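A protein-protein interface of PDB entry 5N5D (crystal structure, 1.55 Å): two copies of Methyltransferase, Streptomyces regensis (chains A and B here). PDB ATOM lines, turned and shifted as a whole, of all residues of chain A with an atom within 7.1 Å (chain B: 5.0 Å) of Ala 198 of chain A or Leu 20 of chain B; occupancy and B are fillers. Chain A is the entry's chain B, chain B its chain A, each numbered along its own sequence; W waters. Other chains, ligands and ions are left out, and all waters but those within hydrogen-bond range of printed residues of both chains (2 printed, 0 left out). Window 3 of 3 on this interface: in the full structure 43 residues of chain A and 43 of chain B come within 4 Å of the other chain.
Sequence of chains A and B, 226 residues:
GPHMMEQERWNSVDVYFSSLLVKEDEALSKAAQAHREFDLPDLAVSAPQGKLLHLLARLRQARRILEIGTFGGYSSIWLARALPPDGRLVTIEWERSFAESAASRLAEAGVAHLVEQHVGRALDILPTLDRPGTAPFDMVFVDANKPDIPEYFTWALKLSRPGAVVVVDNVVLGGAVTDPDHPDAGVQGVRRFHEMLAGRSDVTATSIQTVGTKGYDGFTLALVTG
The backbone carbonyl oxygen (O) of Ala 205 of chain A lies close to the backbone carbonyl oxygen (O) of Leu 21 of chain B, at 3.4 Å.
The backbone carbonyl oxygen (O) of Tyr 16 of chain B is in hydrogen-bond range of the side-chain hydroxyl (OG) of Ser 19 of chain B (2.7 Å). ND1 of His 194 of chain A sits at hydrogen-bond distance from O of Val 190 of chain A, at 2.9 Å. OE2 of Glu 195 of chain A is in salt-bridge range of NH2 of Arg 191 of chain A, 3.9 Å away.
Among the printed residues, pairs that only touch across the chains: Ala 198 of chain A with Leu 20 of chain B (3.2 Å), His 194 of chain A with Phe 17 of chain B (3.3 Å), Leu 197 of chain A with Leu 21 of chain B (3.4 Å), Arg 191 of chain A with Tyr 16 of chain B (3.5 Å), His 194 of chain A with Leu 20 of chain B (3.7 Å) and His 194 of chain A with Leu 21 of chain B (3.8 Å).
Of the printed residues of chain B, Arg 191 of chain A touches Tyr 16. Of the printed residues of chain B, Leu 197 of chain A touches Leu 21. Of chain B, only Leu 20 comes within 4 Å of Ala 198 of chain A. Gly 199 of chain A touches none of the printed residues of chain B. Arg 200 of chain A touches none of the printed residues of chain B. Printed residues of chain B within 4 Å of Ala 205 of chain A: Leu 21 (3.4 Å). Of the printed residues of chain A, Tyr 16 of chain B touches Arg 191. The nearest printed residue of chain A that does not touch Tyr 16 of chain B is His 194 of chain A (4.01 Å).
Of the 7 printed residues of chain B, 4 touch a printed residue of chain A. Hydrophobic or aromatic side chains of chain B within 4 Å of the printed part of chain A: Tyr 16, Phe 17, Leu 20 and Leu 21. Along chain B the printed residues that touch a printed residue of chain A span positions 16 to 21. Among the printed residues, 7 pairs touch across the chains. Among the printed residues, no Asp or Glu carboxylate lies within 4 Å of a Lys or Arg side-chain nitrogen of the other chain.
No position is printed for both chains. Of the 7 pairs that touch across the chains among the printed residues, none has its exchanged pair printed and touching as well.
Water W2 lies within hydrogen-bond range of OE2 of Glu 195 of chain A (2.7 Å), OH of Tyr 16 of chain B (2.7 Å) and NH2 of Arg 191 of chain A (3.2 Å). Water W1 lies within hydrogen-bond range of the backbone carbonyl oxygen (O) of Leu 21 of chain B (2.8 Å) and the backbone NH (N) of Ala 205 of chain A (2.9 Å).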
ATOM      1  N   VAL A 190     -18.519  -8.051  10.448  1.00  0.00           N
ATOM      2  CA  VAL A 190     -19.558  -8.296  11.441  1.00  0.00           C
ATOM      3  C   VAL A 190     -19.109  -9.373  12.421  1.00  0.00           C
ATOM      4  O   VAL A 190     -19.315  -9.250  13.635  1.00  0.00           O
ATOM      5  CB  VAL A 190     -20.889  -8.662  10.752  1.00  0.00           C
ATOM      6  CG1 VAL A 190     -21.930  -9.079  11.786  1.00  0.00           C
ATOM      7  CG2 VAL A 190     -21.400  -7.480   9.940  1.00  0.00           C
ATOM      8  N   ARG A 191     -18.476 -10.437  11.921  1.00  0.00           N
ATOM      9  CA  ARG A 191     -17.985 -11.485  12.813  1.00  0.00           C
ATOM     10  C   ARG A 191     -16.955 -10.928  13.785  1.00  0.00           C
ATOM     11  O   ARG A 191     -17.025 -11.171  14.995  1.00  0.00           O
ATOM     12  CB  ARG A 191     -17.388 -12.634  12.004  1.00  0.00           C
ATOM     13  CG  ARG A 191     -18.438 -13.502  11.305  1.00  0.00           C
ATOM     14  CD  ARG A 191     -17.814 -14.605  10.444  1.00  0.00           C
ATOM     15  NE  ARG A 191     -16.821 -15.399  11.170  1.00  0.00           N
ATOM     16  CZ  ARG A 191     -17.104 -16.435  11.952  1.00  0.00           C
ATOM     17  NH1 ARG A 191     -18.357 -16.832  12.140  1.00  0.00           N
ATOM     18  NH2 ARG A 191     -16.116 -17.087  12.547  1.00  0.00           N
ATOM     19  N   ARG A 192     -15.991 -10.164  13.272  1.00  0.00           N
ATOM     20  CA  ARG A 192     -14.952  -9.622  14.142  1.00  0.00           C
ATOM     21  C   ARG A 192     -15.547  -8.701  15.201  1.00  0.00           C
ATOM     22  O   ARG A 192     -15.113  -8.712  16.354  1.00  0.00           O
ATOM     23  CB  ARG A 192     -13.896  -8.898  13.305  1.00  0.00           C
ATOM     24  CG  ARG A 192     -12.762  -8.305  14.140  1.00  0.00           C
ATOM     25  CD  ARG A 192     -11.481  -8.122  13.347  1.00  0.00           C
ATOM     26  NE  ARG A 192     -11.640  -7.169  12.249  1.00  0.00           N
ATOM     27  CZ  ARG A 192     -11.464  -5.854  12.351  1.00  0.00           C
ATOM     28  NH1 ARG A 192     -11.117  -5.305  13.510  1.00  0.00           N
ATOM     29  NH2 ARG A 192     -11.629  -5.081  11.282  1.00  0.00           N
ATOM     30  N   PHE A 193     -16.556  -7.909  14.829  1.00  0.00           N
ATOM     31  CA  PHE A 193     -17.249  -7.046  15.788  1.00  0.00           C
ATOM     32  C   PHE A 193     -17.884  -7.856  16.919  1.00  0.00           C
ATOM     33  O   PHE A 193     -17.763  -7.501  18.100  1.00  0.00           O
ATOM     34  CB  PHE A 193     -18.291  -6.219  15.023  1.00  0.00           C
ATOM     35  CG  PHE A 193     -19.374  -5.620  15.876  1.00  0.00           C
ATOM     36  CD1 PHE A 193     -19.071  -4.752  16.907  1.00  0.00           C
ATOM     37  CD2 PHE A 193     -20.706  -5.892  15.599  1.00  0.00           C
ATOM     38  CE1 PHE A 193     -20.074  -4.189  17.671  1.00  0.00           C
ATOM     39  CE2 PHE A 193     -21.715  -5.330  16.366  1.00  0.00           C
ATOM     40  CZ  PHE A 193     -21.389  -4.474  17.403  1.00  0.00           C
ATOM     41  N   HIS A 194     -18.568  -8.949  16.585  1.00  0.00           N
ATOM     42  CA  HIS A 194     -19.173  -9.764  17.633  1.00  0.00           C
ATOM     43  C   HIS A 194     -18.110 -10.429  18.494  1.00  0.00           C
ATOM     44  O   HIS A 194     -18.280 -10.558  19.711  1.00  0.00           O
ATOM     45  CB  HIS A 194     -20.124 -10.784  17.015  1.00  0.00           C
ATOM     46  CG  HIS A 194     -21.424 -10.178  16.598  1.00  0.00           C
ATOM     47  ND1 HIS A 194     -21.557  -9.426  15.453  1.00  0.00           N
ATOM     48  CD2 HIS A 194     -22.635 -10.165  17.205  1.00  0.00           C
ATOM     49  CE1 HIS A 194     -22.801  -8.986  15.363  1.00  0.00           C
ATOM     50  NE2 HIS A 194     -23.476  -9.428  16.408  1.00  0.00           N
ATOM     51  N   GLU A 195     -17.002 -10.845  17.883  1.00  0.00           N
ATOM     52  CA  GLU A 195     -15.897 -11.399  18.657  1.00  0.00           C
ATOM     53  C   GLU A 195     -15.322 -10.367  19.617  1.00  0.00           C
ATOM     54  O   GLU A 195     -14.947 -10.699  20.751  1.00  0.00           O
ATOM     55  CB  GLU A 195     -14.826 -11.914  17.704  1.00  0.00           C
ATOM     56  CG  GLU A 195     -15.275 -13.108  16.903  1.00  0.00           C
ATOM     57  CD  GLU A 195     -14.352 -13.440  15.755  1.00  0.00           C
ATOM     58  OE1 GLU A 195     -13.269 -12.815  15.643  1.00  0.00           O
ATOM     59  OE2 GLU A 195     -14.720 -14.325  14.955  1.00  0.00           O
ATOM     60  N   MET A 196     -15.232  -9.111  19.178  1.00  0.00           N
ATOM     61  CA  MET A 196     -14.747  -8.047  20.051  1.00  0.00           C
ATOM     62  C   MET A 196     -15.674  -7.847  21.240  1.00  0.00           C
ATOM     63  O   MET A 196     -15.212  -7.662  22.370  1.00  0.00           O
ATOM     64  CB  MET A 196     -14.597  -6.755  19.255  1.00  0.00           C
ATOM     65  CG  MET A 196     -13.442  -6.816  18.287  1.00  0.00           C
ATOM     66  SD  MET A 196     -13.531  -5.590  16.988  1.00  0.00           S
ATOM     67  CE  MET A 196     -13.164  -4.094  17.895  1.00  0.00           C
ATOM     68  N   LEU A 197     -16.987  -7.883  21.008  1.00  0.00           N
ATOM     69  CA  LEU A 197     -17.933  -7.796  22.115  1.00  0.00           C
ATOM     70  C   LEU A 197     -17.731  -8.942  23.100  1.00  0.00           C
ATOM     71  O   LEU A 197     -17.731  -8.730  24.320  1.00  0.00           O
ATOM     72  CB  LEU A 197     -19.366  -7.794  21.587  1.00  0.00           C
ATOM     73  CG  LEU A 197     -19.855  -6.480  20.972  1.00  0.00           C
ATOM     74  CD1 LEU A 197     -21.149  -6.686  20.197  1.00  0.00           C
ATOM     75  CD2 LEU A 197     -20.052  -5.422  22.059  1.00  0.00           C
ATOM     76  N   ALA A 198     -17.540 -10.159  22.592  1.00  0.00           N
ATOM     77  CA  ALA A 198     -17.295 -11.295  23.475  1.00  0.00           C
ATOM     78  C   ALA A 198     -16.044 -11.087  24.314  1.00  0.00           C
ATOM     79  O   ALA A 198     -15.999 -11.507  25.473  1.00  0.00           O
ATOM     80  CB  ALA A 198     -17.151 -12.582  22.666  1.00  0.00           C
ATOM     81  N   GLY A 199     -15.034 -10.443  23.747  1.00  0.00           N
ATOM     82  CA  GLY A 199     -13.725 -10.347  24.351  1.00  0.00           C
ATOM     83  C   GLY A 199     -13.502  -9.179  25.278  1.00  0.00           C
ATOM     84  O   GLY A 199     -12.370  -8.982  25.724  1.00  0.00           O
ATOM     85  N   ARG A 200     -14.531  -8.399  25.604  1.00  0.00           N
ATOM     86  CA  ARG A 200     -14.350  -7.313  26.552  1.00  0.00           C
ATOM     87  C   ARG A 200     -15.583  -7.196  27.432  1.00  0.00           C
ATOM     88  O   ARG A 200     -16.667  -7.681  27.092  1.00  0.00           O
ATOM     89  CB  ARG A 200     -14.048  -5.983  25.841  1.00  0.00           C
ATOM     90  CG  ARG A 200     -15.153  -5.460  24.947  1.00  0.00           C
ATOM     91  CD  ARG A 200     -14.595  -4.382  24.024  1.00  0.00           C
ATOM     92  NE  ARG A 200     -14.126  -3.221  24.774  1.00  0.00           N
ATOM     93  CZ  ARG A 200     -13.227  -2.341  24.341  1.00  0.00           C
ATOM     94  NH1 ARG A 200     -12.877  -1.321  25.112  1.00  0.00           N
ATOM     95  NH2 ARG A 200     -12.664  -2.474  23.148  1.00  0.00           N
ATOM     96  N   SER A 201     -15.390  -6.539  28.578  1.00  0.00           N
ATOM     97  CA  SER A 201     -16.380  -6.520  29.640  1.00  0.00           C
ATOM     98  C   SER A 201     -16.883  -5.126  29.979  1.00  0.00           C
ATOM     99  O   SER A 201     -17.707  -4.995  30.889  1.00  0.00           O
ATOM    100  CB  SER A 201     -15.804  -7.165  30.904  1.00  0.00           C
ATOM    101  OG  SER A 201     -15.454  -8.512  30.653  1.00  0.00           O
ATOM    102  N   VAL A 203     -18.594  -3.309  27.937  1.00  0.00           N
ATOM    103  CA  VAL A 203     -19.773  -3.115  27.109  1.00  0.00           C
ATOM    104  C   VAL A 203     -20.485  -4.457  27.060  1.00  0.00           C
ATOM    105  O   VAL A 203     -19.857  -5.514  27.173  1.00  0.00           O
ATOM    106  CB  VAL A 203     -19.399  -2.580  25.704  1.00  0.00           C
ATOM    107  CG1 VAL A 203     -18.286  -3.400  25.093  1.00  0.00           C
ATOM    108  CG2 VAL A 203     -20.622  -2.534  24.777  1.00  0.00           C
ATOM    109  N   ALA A 205     -24.076  -6.584  25.279  1.00  0.00           N
ATOM    110  CA  ALA A 205     -24.865  -6.442  24.066  1.00  0.00           C
ATOM    111  C   ALA A 205     -25.754  -7.656  23.817  1.00  0.00           C
ATOM    112  O   ALA A 205     -25.643  -8.699  24.470  1.00  0.00           O
ATOM    113  CB  ALA A 205     -23.951  -6.209  22.859  1.00  0.00           C
ATOM    114  N   TYR B  16     -25.281 -18.559  17.343  1.00  0.00           N
ATOM    115  CA  TYR B  16     -24.021 -17.876  17.064  1.00  0.00           C
ATOM    116  C   TYR B  16     -23.929 -16.558  17.824  1.00  0.00           C
ATOM    117  O   TYR B  16     -22.959 -16.309  18.547  1.00  0.00           O
ATOM    118  CB  TYR B  16     -23.868 -17.637  15.558  1.00  0.00           C
ATOM    119  CG  TYR B  16     -22.751 -16.664  15.265  1.00  0.00           C
ATOM    120  CD1 TYR B  16     -21.422 -17.068  15.298  1.00  0.00           C
ATOM    121  CD2 TYR B  16     -23.023 -15.339  14.987  1.00  0.00           C
ATOM    122  CE1 TYR B  16     -20.403 -16.169  15.058  1.00  0.00           C
ATOM    123  CE2 TYR B  16     -22.012 -14.433  14.744  1.00  0.00           C
ATOM    124  CZ  TYR B  16     -20.705 -14.849  14.785  1.00  0.00           C
ATOM    125  OH  TYR B  16     -19.727 -13.912  14.543  1.00  0.00           O
ATOM    126  N   PHE B  17     -24.922 -15.685  17.662  1.00  0.00           N
ATOM    127  CA  PHE B  17     -24.900 -14.411  18.376  1.00  0.00           C
ATOM    128  C   PHE B  17     -24.878 -14.633  19.880  1.00  0.00           C
ATOM    129  O   PHE B  17     -24.101 -14.002  20.606  1.00  0.00           O
ATOM    130  CB  PHE B  17     -26.119 -13.566  17.998  1.00  0.00           C
ATOM    131  CG  PHE B  17     -26.079 -12.976  16.615  1.00  0.00           C
ATOM    132  CD1 PHE B  17     -24.911 -12.490  16.066  1.00  0.00           C
ATOM    133  CD2 PHE B  17     -27.250 -12.873  15.880  1.00  0.00           C
ATOM    134  CE1 PHE B  17     -24.903 -11.933  14.793  1.00  0.00           C
ATOM    135  CE2 PHE B  17     -27.247 -12.325  14.616  1.00  0.00           C
ATOM    136  CZ  PHE B  17     -26.072 -11.859  14.070  1.00  0.00           C
ATOM    137  N   SER B  18     -25.733 -15.535  20.363  1.00  0.00           N
ATOM    138  CA  SER B  18     -25.801 -15.845  21.789  1.00  0.00           C
ATOM    139  C   SER B  18     -24.451 -16.300  22.329  1.00  0.00           C
ATOM    140  O   SER B  18     -24.039 -15.891  23.423  1.00  0.00           O
ATOM    141  CB  SER B  18     -26.848 -16.933  22.029  1.00  0.00           C
ATOM    142  OG  SER B  18     -27.931 -16.444  22.785  1.00  0.00           O
ATOM    143  N   SER B  19     -23.760 -17.169  21.586  1.00  0.00           N
ATOM    144  CA  SER B  19     -22.494 -17.717  22.057  1.00  0.00           C
ATOM    145  C   SER B  19     -21.487 -16.621  22.363  1.00  0.00           C
ATOM    146  O   SER B  19     -20.653 -16.778  23.264  1.00  0.00           O
ATOM    147  CB  SER B  19     -21.915 -18.692  21.022  1.00  0.00           C
ATOM    148  OG  SER B  19     -21.326 -18.027  19.911  1.00  0.00           O
ATOM    149  N   LEU B  20     -21.541 -15.513  21.633  1.00  0.00           N
ATOM    150  CA  LEU B  20     -20.592 -14.431  21.818  1.00  0.00           C
ATOM    151  C   LEU B  20     -21.103 -13.343  22.744  1.00  0.00           C
ATOM    152  O   LEU B  20     -20.294 -12.686  23.412  1.00  0.00           O
ATOM    153  CB  LEU B  20     -20.225 -13.816  20.461  1.00  0.00           C
ATOM    154  CG  LEU B  20     -19.452 -14.782  19.542  1.00  0.00           C
ATOM    155  CD1 LEU B  20     -19.339 -14.264  18.121  1.00  0.00           C
ATOM    156  CD2 LEU B  20     -18.053 -15.013  20.100  1.00  0.00           C
ATOM    157  N   LEU B  21     -22.424 -13.138  22.822  1.00  0.00           N
ATOM    158  CA  LEU B  21     -22.947 -11.963  23.510  1.00  0.00           C
ATOM    159  C   LEU B  21     -23.681 -12.241  24.815  1.00  0.00           C
ATOM    160  O   LEU B  21     -23.764 -11.332  25.648  1.00  0.00           O
ATOM    161  CB  LEU B  21     -23.904 -11.190  22.593  1.00  0.00           C
ATOM    162  CG  LEU B  21     -23.324 -10.671  21.278  1.00  0.00           C
ATOM    163  CD1 LEU B  21     -24.361  -9.791  20.576  1.00  0.00           C
ATOM    164  CD2 LEU B  21     -22.029  -9.919  21.456  1.00  0.00           C
ATOM    165  N   VAL B  22     -24.233 -13.435  25.016  1.00  0.00           N
ATOM    166  CA  VAL B  22     -25.154 -13.673  26.123  1.00  0.00           C
ATOM    167  C   VAL B  22     -24.666 -14.861  26.939  1.00  0.00           C
ATOM    168  O   VAL B  22     -24.565 -15.978  26.418  1.00  0.00           O
ATOM    169  CB  VAL B  22     -26.586 -13.918  25.629  1.00  0.00           C
ATOM    170  CG1 VAL B  22     -27.548 -13.996  26.815  1.00  0.00           C
ATOM    171  CG2 VAL B  22     -27.006 -12.831  24.654  1.00  0.00           C
HETATM  172  O   HOH W   1     -22.371  -8.861  25.463  1.00  0.00           O
HETATM  173  O   HOH W   2     -17.284 -15.035  14.703  1.00  0.00           O
